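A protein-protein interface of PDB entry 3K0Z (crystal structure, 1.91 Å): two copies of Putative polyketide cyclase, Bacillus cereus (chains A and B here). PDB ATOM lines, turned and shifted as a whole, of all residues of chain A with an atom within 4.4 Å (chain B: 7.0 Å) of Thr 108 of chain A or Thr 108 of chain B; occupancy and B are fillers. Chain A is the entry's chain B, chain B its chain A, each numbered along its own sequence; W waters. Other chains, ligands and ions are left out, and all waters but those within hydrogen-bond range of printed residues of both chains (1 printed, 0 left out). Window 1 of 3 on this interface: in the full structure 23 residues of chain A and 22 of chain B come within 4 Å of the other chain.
Of the 17 printed residues of chain B, 6 touch a printed residue of chain A.
Of the 10 printed residues of chain A, 6 touch a printed residue of chain B.
Printed residues of chain A that touch a printed residue of chain B: Asp 99, Leu 101, Thr 108, Arg 110, Ile 127 and Ile 129.
Among the printed residues, 12 pairs touch across the chains.
Leu 101 of chain A touches Thr 108 of chain B, and with the chains exchanged Thr 108 of chain A touches Leu 101 of chain B.
Thr 108 of chain B touches its own counterpart, Thr 108 of chain A.
Thr 108 of chain A touches Ile 129 of chain B, and with the chains exchanged Ile 129 of chain A touches Thr 108 of chain B.
Ile 129 of chain A touches Leu 101 of chain B, but with the chains exchanged Leu 101 of chain A does not touch Ile 129 of chain B (4.02 Å).
Of the 12 pairs that touch across the chains among the printed residues, 8 have their exchanged pair printed and touching as well.
NZ of Lys 106 of chain B is in salt-bridge range of OD2 of Asp 99 of chain A (2.8 Å).
The side-chain hydroxyl of Thr 108 of chain B lies within hydrogen-bond range of the side-chain hydroxyl of Thr 108 of chain A (2.9 Å).
Lys 106 of chain B touches Leu 101 of chain A (CG to CD2, 3.97 Å).
Leu 101 of chain A touches Thr 108 of chain B (CD1 to OG1, 3.6 Å).
Thr 108 of chain A touches Leu 101 of chain B.
Ile 129 of chain B touches Thr 108 of chain A.
Ile 129 of chain B touches Arg 110 of chain A (CD1 to CB, 3.9 Å).
Ile 127 of chain B touches Ile 127 of chain A.
CG2 of Ile 129 of chain A touches CD1 of Leu 101 of chain B, at 3.96 Å.
Ile 129 of chain A touches Thr 108 of chain B.
Arg 110 of chain B touches Ile 129 of chain A (CB to CD1, 3.9 Å).
Ile 127 of chain B touches Ile 129 of chain A.
The backbone NH (N) of Thr 108 of chain A lies within hydrogen-bond range of the backbone carbonyl oxygen (O) of Leu 101 of chain A, at 2.9 Å.
The backbone carbonyl oxygen (O) of Thr 108 of chain B is in hydrogen-bond range of the backbone NH (N) of Leu 101 of chain B (2.8 Å).
The backbone NH (N) of Arg 110 of chain B lies within hydrogen-bond range of the backbone carbonyl oxygen (O) of Asp 99 of chain B, at 2.9 Å.
N of Arg 110 of chain A lies within hydrogen-bond range of O of Asp 99 of chain A (2.9 Å).
Printed residues of chain A within 4 Å of Lys 106 of chain B: Asp 99 and Leu 101.
Of chain A, only Leu 101, Thr 108 and Ile 129 come within 4 Å of Thr 108 of chain B.
Printed residues of chain A within 4 Å of Ile 127 of chain B: Ile 127 (3.6 Å) and Ile 129 (3.9 Å).
The nearest residue of chain B that does not touch Thr 108 of chain A is Ile 127 of chain B (5.4 Å).
Water W1 lies within hydrogen-bond range of OD1 of Asp 99 of chain A (2.6 Å) and NZ of Lys 106 of chain B (2.8 Å).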
ATOM      1  N   ASP A  99      14.606 -22.898  19.139  1.00  0.00           N
ATOM      2  CA  ASP A  99      14.440 -21.435  19.266  1.00  0.00           C
ATOM      3  C   ASP A  99      15.570 -20.818  18.441  1.00  0.00           C
ATOM      4  O   ASP A  99      16.687 -21.385  18.371  1.00  0.00           O
ATOM      5  CB  ASP A  99      14.606 -21.004  20.701  1.00  0.00           C
ATOM      6  CG  ASP A  99      14.009 -19.646  21.000  1.00  0.00           C
ATOM      7  OD1 ASP A  99      13.452 -18.994  20.083  1.00  0.00           O
ATOM      8  OD2 ASP A  99      14.124 -19.228  22.180  1.00  0.00           O
ATOM      9  N   LEU A 100      15.236 -19.733  17.756  1.00  0.00           N
ATOM     10  CA  LEU A 100      16.174 -18.983  16.899  1.00  0.00           C
ATOM     11  C   LEU A 100      16.003 -17.515  17.206  1.00  0.00           C
ATOM     12  O   LEU A 100      14.886 -16.980  17.118  1.00  0.00           O
ATOM     13  CB  LEU A 100      15.876 -19.255  15.402  1.00  0.00           C
ATOM     14  CG  LEU A 100      16.999 -18.937  14.390  1.00  0.00           C
ATOM     15  CD1 LEU A 100      18.208 -19.865  14.609  1.00  0.00           C
ATOM     16  CD2 LEU A 100      16.480 -19.015  12.948  1.00  0.00           C
ATOM     17  N   LEU A 101      17.112 -16.857  17.553  1.00  0.00           N
ATOM     18  CA  LEU A 101      17.132 -15.447  18.018  1.00  0.00           C
ATOM     19  C   LEU A 101      18.096 -14.665  17.105  1.00  0.00           C
ATOM     20  O   LEU A 101      19.306 -14.860  17.171  1.00  0.00           O
ATOM     21  CB  LEU A 101      17.595 -15.377  19.499  1.00  0.00           C
ATOM     22  CG  LEU A 101      16.879 -16.300  20.495  1.00  0.00           C
ATOM     23  CD1 LEU A 101      17.546 -16.222  21.871  1.00  0.00           C
ATOM     24  CD2 LEU A 101      15.335 -16.055  20.535  1.00  0.00           C
ATOM     25  N   VAL A 107      23.237 -14.662  15.508  1.00  0.00           N
ATOM     26  CA  VAL A 107      22.115 -15.605  15.637  1.00  0.00           C
ATOM     27  C   VAL A 107      22.376 -16.573  16.780  1.00  0.00           C
ATOM     28  O   VAL A 107      23.448 -17.163  16.833  1.00  0.00           O
ATOM     29  CB  VAL A 107      21.910 -16.419  14.340  1.00  0.00           C
ATOM     30  CG1 VAL A 107      20.786 -17.480  14.546  1.00  0.00           C
ATOM     31  CG2 VAL A 107      21.550 -15.468  13.155  1.00  0.00           C
ATOM     32  N   THR A 108      21.418 -16.712  17.708  1.00  0.00           N
ATOM     33  CA  THR A 108      21.459 -17.787  18.685  1.00  0.00           C
ATOM     34  C   THR A 108      20.499 -18.889  18.255  1.00  0.00           C
ATOM     35  O   THR A 108      19.344 -18.618  17.924  1.00  0.00           O
ATOM     36  CB  THR A 108      21.064 -17.307  20.091  1.00  0.00           C
ATOM     37  OG1 THR A 108      21.930 -16.251  20.464  1.00  0.00           O
ATOM     38  CG2 THR A 108      21.122 -18.442  21.170  1.00  0.00           C
ATOM     39  N   ALA A 109      20.980 -20.132  18.259  1.00  0.00           N
ATOM     40  CA  ALA A 109      20.127 -21.282  18.039  1.00  0.00           C
ATOM     41  C   ALA A 109      20.131 -22.167  19.274  1.00  0.00           C
ATOM     42  O   ALA A 109      21.201 -22.435  19.844  1.00  0.00           O
ATOM     43  CB  ALA A 109      20.608 -22.069  16.821  1.00  0.00           C
ATOM     44  N   ARG A 110      18.948 -22.644  19.688  1.00  0.00           N
ATOM     45  CA  ARG A 110      18.866 -23.726  20.694  1.00  0.00           C
ATOM     46  C   ARG A 110      18.371 -24.947  19.955  1.00  0.00           C
ATOM     47  O   ARG A 110      17.345 -24.869  19.293  1.00  0.00           O
ATOM     48  CB  ARG A 110      17.937 -23.385  21.858  1.00  0.00           C
ATOM     49  CG  ARG A 110      17.760 -24.522  22.856  1.00  0.00           C
ATOM     50  CD  ARG A 110      17.119 -24.041  24.134  1.00  0.00           C
ATOM     51  NE  ARG A 110      15.751 -23.567  23.932  1.00  0.00           N
ATOM     52  CZ  ARG A 110      14.692 -24.364  23.877  1.00  0.00           C
ATOM     53  NH1 ARG A 110      14.824 -25.671  23.989  1.00  0.00           N
ATOM     54  NH2 ARG A 110      13.490 -23.854  23.701  1.00  0.00           N
ATOM     55  N   ILE A 127      23.446 -25.334  22.341  1.00  0.00           N
ATOM     56  CA  ILE A 127      23.214 -23.915  22.114  1.00  0.00           C
ATOM     57  C   ILE A 127      24.420 -23.386  21.337  1.00  0.00           C
ATOM     58  O   ILE A 127      25.572 -23.654  21.712  1.00  0.00           O
ATOM     59  CB  ILE A 127      23.029 -23.051  23.398  1.00  0.00           C
ATOM     60  CG1 ILE A 127      21.877 -23.560  24.283  1.00  0.00           C
ATOM     61  CG2 ILE A 127      22.806 -21.602  23.001  1.00  0.00           C
ATOM     62  CD1 ILE A 127      21.765 -22.905  25.671  1.00  0.00           C
ATOM     63  N   ASP A 128      24.132 -22.660  20.258  1.00  0.00           N
ATOM     64  CA  ASP A 128      25.142 -22.070  19.411  1.00  0.00           C
ATOM     65  C   ASP A 128      24.875 -20.590  19.246  1.00  0.00           C
ATOM     66  O   ASP A 128      23.699 -20.155  19.208  1.00  0.00           O
ATOM     67  CB  ASP A 128      25.051 -22.668  18.014  1.00  0.00           C
ATOM     68  CG  ASP A 128      25.241 -24.196  17.980  1.00  0.00           C
ATOM     69  OD1 ASP A 128      25.413 -24.832  19.040  1.00  0.00           O
ATOM     70  OD2 ASP A 128      25.225 -24.755  16.849  1.00  0.00           O
ATOM     71  N   ILE A 129      25.958 -19.849  19.069  1.00  0.00           N
ATOM     72  CA  ILE A 129      25.944 -18.434  18.688  1.00  0.00           C
ATOM     73  C   ILE A 129      26.709 -18.344  17.341  1.00  0.00           C
ATOM     74  O   ILE A 129      27.865 -18.740  17.271  1.00  0.00           O
ATOM     75  CB  ILE A 129      26.656 -17.549  19.741  1.00  0.00           C
ATOM     76  CG1 ILE A 129      25.839 -17.515  21.043  1.00  0.00           C
ATOM     77  CG2 ILE A 129      26.859 -16.125  19.202  1.00  0.00           C
ATOM     78  CD1 ILE A 129      26.602 -16.988  22.326  1.00  0.00           C
ATOM     79  N   TYR B  44      24.678 -12.531  36.458  1.00  0.00           N
ATOM     80  CA  TYR B  44      26.093 -12.971  36.482  1.00  0.00           C
ATOM     81  C   TYR B  44      26.882 -12.422  37.694  1.00  0.00           C
ATOM     82  O   TYR B  44      27.850 -13.064  38.104  1.00  0.00           O
ATOM     83  CB  TYR B  44      26.798 -12.849  35.113  1.00  0.00           C
ATOM     84  CG  TYR B  44      25.971 -13.653  34.142  1.00  0.00           C
ATOM     85  CD1 TYR B  44      25.916 -15.038  34.241  1.00  0.00           C
ATOM     86  CD2 TYR B  44      25.137 -13.027  33.238  1.00  0.00           C
ATOM     87  CE1 TYR B  44      25.038 -15.801  33.466  1.00  0.00           C
ATOM     88  CE2 TYR B  44      24.284 -13.783  32.415  1.00  0.00           C
ATOM     89  CZ  TYR B  44      24.248 -15.164  32.547  1.00  0.00           C
ATOM     90  OH  TYR B  44      23.391 -15.891  31.780  1.00  0.00           O
ATOM     91  N   ILE B  97      31.161 -11.880  31.572  1.00  0.00           N
ATOM     92  CA  ILE B  97      30.268 -11.910  30.434  1.00  0.00           C
ATOM     93  C   ILE B  97      31.079 -11.551  29.165  1.00  0.00           C
ATOM     94  O   ILE B  97      31.570 -10.396  28.989  1.00  0.00           O
ATOM     95  CB  ILE B  97      29.070 -10.879  30.606  1.00  0.00           C
ATOM     96  CG1 ILE B  97      28.288 -11.091  31.912  1.00  0.00           C
ATOM     97  CG2 ILE B  97      28.136 -10.881  29.343  1.00  0.00           C
ATOM     98  CD1 ILE B  97      27.270  -9.937  32.223  1.00  0.00           C
ATOM     99  N   ASP B  99      29.830 -11.979  25.935  1.00  0.00           N
ATOM    100  CA  ASP B  99      28.994 -11.415  24.890  1.00  0.00           C
ATOM    101  C   ASP B  99      27.539 -11.478  25.377  1.00  0.00           C
ATOM    102  O   ASP B  99      27.165 -12.387  26.116  1.00  0.00           O
ATOM    103  CB  ASP B  99      29.238 -12.169  23.588  1.00  0.00           C
ATOM    104  CG  ASP B  99      28.687 -11.450  22.330  1.00  0.00           C
ATOM    105  OD1 ASP B  99      28.224 -10.294  22.399  1.00  0.00           O
ATOM    106  OD2 ASP B  99      28.710 -12.107  21.252  1.00  0.00           O
ATOM    107  N   LEU B 100      26.787 -10.435  25.072  1.00  0.00           N
ATOM    108  CA  LEU B 100      25.383 -10.338  25.391  1.00  0.00           C
ATOM    109  C   LEU B 100      24.574  -9.929  24.167  1.00  0.00           C
ATOM    110  O   LEU B 100      24.808  -8.834  23.596  1.00  0.00           O
ATOM    111  CB  LEU B 100      25.209  -9.295  26.498  1.00  0.00           C
ATOM    112  CG  LEU B 100      24.097  -9.476  27.485  1.00  0.00           C
ATOM    113  CD1 LEU B 100      24.302 -10.815  28.324  1.00  0.00           C
ATOM    114  CD2 LEU B 100      23.946  -8.213  28.360  1.00  0.00           C
ATOM    115  N   LEU B 101      23.605 -10.757  23.772  1.00  0.00           N
ATOM    116  CA  LEU B 101      22.744 -10.496  22.555  1.00  0.00           C
ATOM    117  C   LEU B 101      21.315 -10.249  23.038  1.00  0.00           C
ATOM    118  O   LEU B 101      20.684 -11.144  23.637  1.00  0.00           O
ATOM    119  CB  LEU B 101      22.770 -11.669  21.604  1.00  0.00           C
ATOM    120  CG  LEU B 101      24.207 -12.170  21.413  1.00  0.00           C
ATOM    121  CD1 LEU B 101      24.210 -13.535  20.603  1.00  0.00           C
ATOM    122  CD2 LEU B 101      25.079 -11.062  20.770  1.00  0.00           C
ATOM    123  N   VAL B 102      20.805  -9.046  22.782  1.00  0.00           N
ATOM    124  CA  VAL B 102      19.507  -8.624  23.364  1.00  0.00           C
ATOM    125  C   VAL B 102      18.463  -8.373  22.276  1.00  0.00           C
ATOM    126  O   VAL B 102      18.631  -7.498  21.470  1.00  0.00           O
ATOM    127  CB  VAL B 102      19.694  -7.399  24.272  1.00  0.00           C
ATOM    128  CG1 VAL B 102      18.392  -7.047  24.936  1.00  0.00           C
ATOM    129  CG2 VAL B 102      20.843  -7.658  25.340  1.00  0.00           C
ATOM    130  N   VAL B 103      17.367  -9.150  22.267  1.00  0.00           N
ATOM    131  CA  VAL B 103      16.365  -9.026  21.207  1.00  0.00           C
ATOM    132  C   VAL B 103      15.015  -9.498  21.656  1.00  0.00           C
ATOM    133  O   VAL B 103      14.908 -10.516  22.323  1.00  0.00           O
ATOM    134  CB  VAL B 103      16.817  -9.785  19.927  1.00  0.00           C
ATOM    135  CG1 VAL B 103      16.919 -11.337  20.134  1.00  0.00           C
ATOM    136  CG2 VAL B 103      15.905  -9.410  18.695  1.00  0.00           C
ATOM    137  N   LYS B 106      14.280 -11.722  24.896  1.00  0.00           N
ATOM    138  CA  LYS B 106      15.301 -12.746  25.126  1.00  0.00           C
ATOM    139  C   LYS B 106      16.703 -12.137  25.205  1.00  0.00           C
ATOM    140  O   LYS B 106      17.023 -11.123  24.549  1.00  0.00           O
ATOM    141  CB  LYS B 106      15.228 -13.830  24.027  1.00  0.00           C
ATOM    142  CG  LYS B 106      13.925 -14.683  23.980  1.00  0.00           C
ATOM    143  CD  LYS B 106      14.060 -16.055  24.540  1.00  0.00           C
ATOM    144  CE  LYS B 106      12.716 -16.815  24.523  1.00  0.00           C
ATOM    145  NZ  LYS B 106      12.270 -17.399  23.222  1.00  0.00           N
ATOM    146  N   VAL B 107      17.531 -12.728  26.064  1.00  0.00           N
ATOM    147  CA  VAL B 107      18.935 -12.318  26.186  1.00  0.00           C
ATOM    148  C   VAL B 107      19.792 -13.578  26.064  1.00  0.00           C
ATOM    149  O   VAL B 107      19.545 -14.546  26.747  1.00  0.00           O
ATOM    150  CB  VAL B 107      19.238 -11.638  27.559  1.00  0.00           C
ATOM    151  CG1 VAL B 107      20.765 -11.312  27.706  1.00  0.00           C
ATOM    152  CG2 VAL B 107      18.461 -10.379  27.716  1.00  0.00           C
ATOM    153  N   THR B 108      20.783 -13.569  25.185  1.00  0.00           N
ATOM    154  CA  THR B 108      21.759 -14.658  25.149  1.00  0.00           C
ATOM    155  C   THR B 108      23.019 -14.138  25.778  1.00  0.00           C
ATOM    156  O   THR B 108      23.474 -13.056  25.396  1.00  0.00           O
ATOM    157  CB  THR B 108      22.099 -15.044  23.731  1.00  0.00           C
ATOM    158  OG1 THR B 108      20.887 -15.396  23.029  1.00  0.00           O
ATOM    159  CG2 THR B 108      23.094 -16.221  23.751  1.00  0.00           C
ATOM    160  N   ALA B 109      23.561 -14.882  26.731  1.00  0.00           N
ATOM    161  CA  ALA B 109      24.839 -14.548  27.346  1.00  0.00           C
ATOM    162  C   ALA B 109      25.843 -15.648  27.086  1.00  0.00           C
ATOM    163  O   ALA B 109      25.501 -16.844  27.242  1.00  0.00           O
ATOM    164  CB  ALA B 109      24.688 -14.324  28.913  1.00  0.00           C
ATOM    165  N   ARG B 110      27.071 -15.254  26.723  1.00  0.00           N
ATOM    166  CA  ARG B 110      28.168 -16.182  26.650  1.00  0.00           C
ATOM    167  C   ARG B 110      29.118 -15.824  27.788  1.00  0.00           C
ATOM    168  O   ARG B 110      29.624 -14.683  27.863  1.00  0.00           O
ATOM    169  CB  ARG B 110      28.891 -16.107  25.302  1.00  0.00           C
ATOM    170  CG  ARG B 110      30.082 -17.009  25.170  1.00  0.00           C
ATOM    171  CD  ARG B 110      30.613 -17.093  23.706  1.00  0.00           C
ATOM    172  NE  ARG B 110      31.155 -15.839  23.188  1.00  0.00           N
ATOM    173  CZ  ARG B 110      32.379 -15.392  23.416  1.00  0.00           C
ATOM    174  NH1 ARG B 110      33.197 -16.032  24.221  1.00  0.00           N
ATOM    175  NH2 ARG B 110      32.772 -14.255  22.857  1.00  0.00           N
ATOM    176  N   LEU B 111      29.386 -16.796  28.634  1.00  0.00           N
ATOM    177  CA  LEU B 111      30.177 -16.598  29.854  1.00  0.00           C
ATOM    178  C   LEU B 111      31.533 -17.274  29.844  1.00  0.00           C
ATOM    179  O   LEU B 111      31.733 -18.254  29.108  1.00  0.00           O
ATOM    180  CB  LEU B 111      29.394 -17.137  31.053  1.00  0.00           C
ATOM    181  CG  LEU B 111      27.992 -16.560  31.368  1.00  0.00           C
ATOM    182  CD1 LEU B 111      27.895 -14.967  31.238  1.00  0.00           C
ATOM    183  CD2 LEU B 111      26.847 -17.273  30.601  1.00  0.00           C
ATOM    184  N   ILE B 127      26.933 -20.943  27.798  1.00  0.00           N
ATOM    185  CA  ILE B 127      25.991 -20.108  27.031  1.00  0.00           C
ATOM    186  C   ILE B 127      24.601 -20.256  27.667  1.00  0.00           C
ATOM    187  O   ILE B 127      24.156 -21.395  27.943  1.00  0.00           O
ATOM    188  CB  ILE B 127      25.890 -20.472  25.510  1.00  0.00           C
ATOM    189  CG1 ILE B 127      27.268 -20.483  24.834  1.00  0.00           C
ATOM    190  CG2 ILE B 127      24.957 -19.460  24.847  1.00  0.00           C
ATOM    191  CD1 ILE B 127      27.292 -20.989  23.378  1.00  0.00           C
ATOM    192  N   ASP B 128      23.929 -19.121  27.905  1.00  0.00           N
ATOM    193  CA  ASP B 128      22.622 -19.111  28.528  1.00  0.00           C
ATOM    194  C   ASP B 128      21.670 -18.322  27.677  1.00  0.00           C
ATOM    195  O   ASP B 128      22.053 -17.305  27.101  1.00  0.00           O
ATOM    196  CB  ASP B 128      22.610 -18.389  29.875  1.00  0.00           C
ATOM    197  CG  ASP B 128      23.532 -18.992  30.933  1.00  0.00           C
ATOM    198  OD1 ASP B 128      24.331 -19.933  30.657  1.00  0.00           O
ATOM    199  OD2 ASP B 128      23.428 -18.520  32.096  1.00  0.00           O
ATOM    200  N   ILE B 129      20.429 -18.773  27.627  1.00  0.00           N
ATOM    201  CA  ILE B 129      19.345 -18.026  26.998  1.00  0.00           C
ATOM    202  C   ILE B 129      18.374 -17.676  28.139  1.00  0.00           C
ATOM    203  O   ILE B 129      17.844 -18.566  28.825  1.00  0.00           O
ATOM    204  CB  ILE B 129      18.605 -18.826  25.927  1.00  0.00           C
ATOM    205  CG1 ILE B 129      19.554 -19.125  24.752  1.00  0.00           C
ATOM    206  CG2 ILE B 129      17.370 -18.022  25.457  1.00  0.00           C
ATOM    207  CD1 ILE B 129      19.057 -20.224  23.828  1.00  0.00           C
ATOM    208  N   LEU B 130      18.171 -16.382  28.320  1.00  0.00           N
ATOM    209  CA  LEU B 130      17.303 -15.856  29.377  1.00  0.00           C
ATOM    210  C   LEU B 130      16.035 -15.236  28.796  1.00  0.00           C
ATOM    211  O   LEU B 130      16.119 -14.492  27.842  1.00  0.00           O
ATOM    212  CB  LEU B 130      18.057 -14.780  30.127  1.00  0.00           C
ATOM    213  CG  LEU B 130      19.464 -15.057  30.650  1.00  0.00           C
ATOM    214  CD1 LEU B 130      20.022 -13.709  31.160  1.00  0.00           C
ATOM    215  CD2 LEU B 130      19.569 -16.136  31.724  1.00  0.00           C
HETATM  216  O   HOH W   1      11.934 -16.882  20.515  1.00  0.00           O
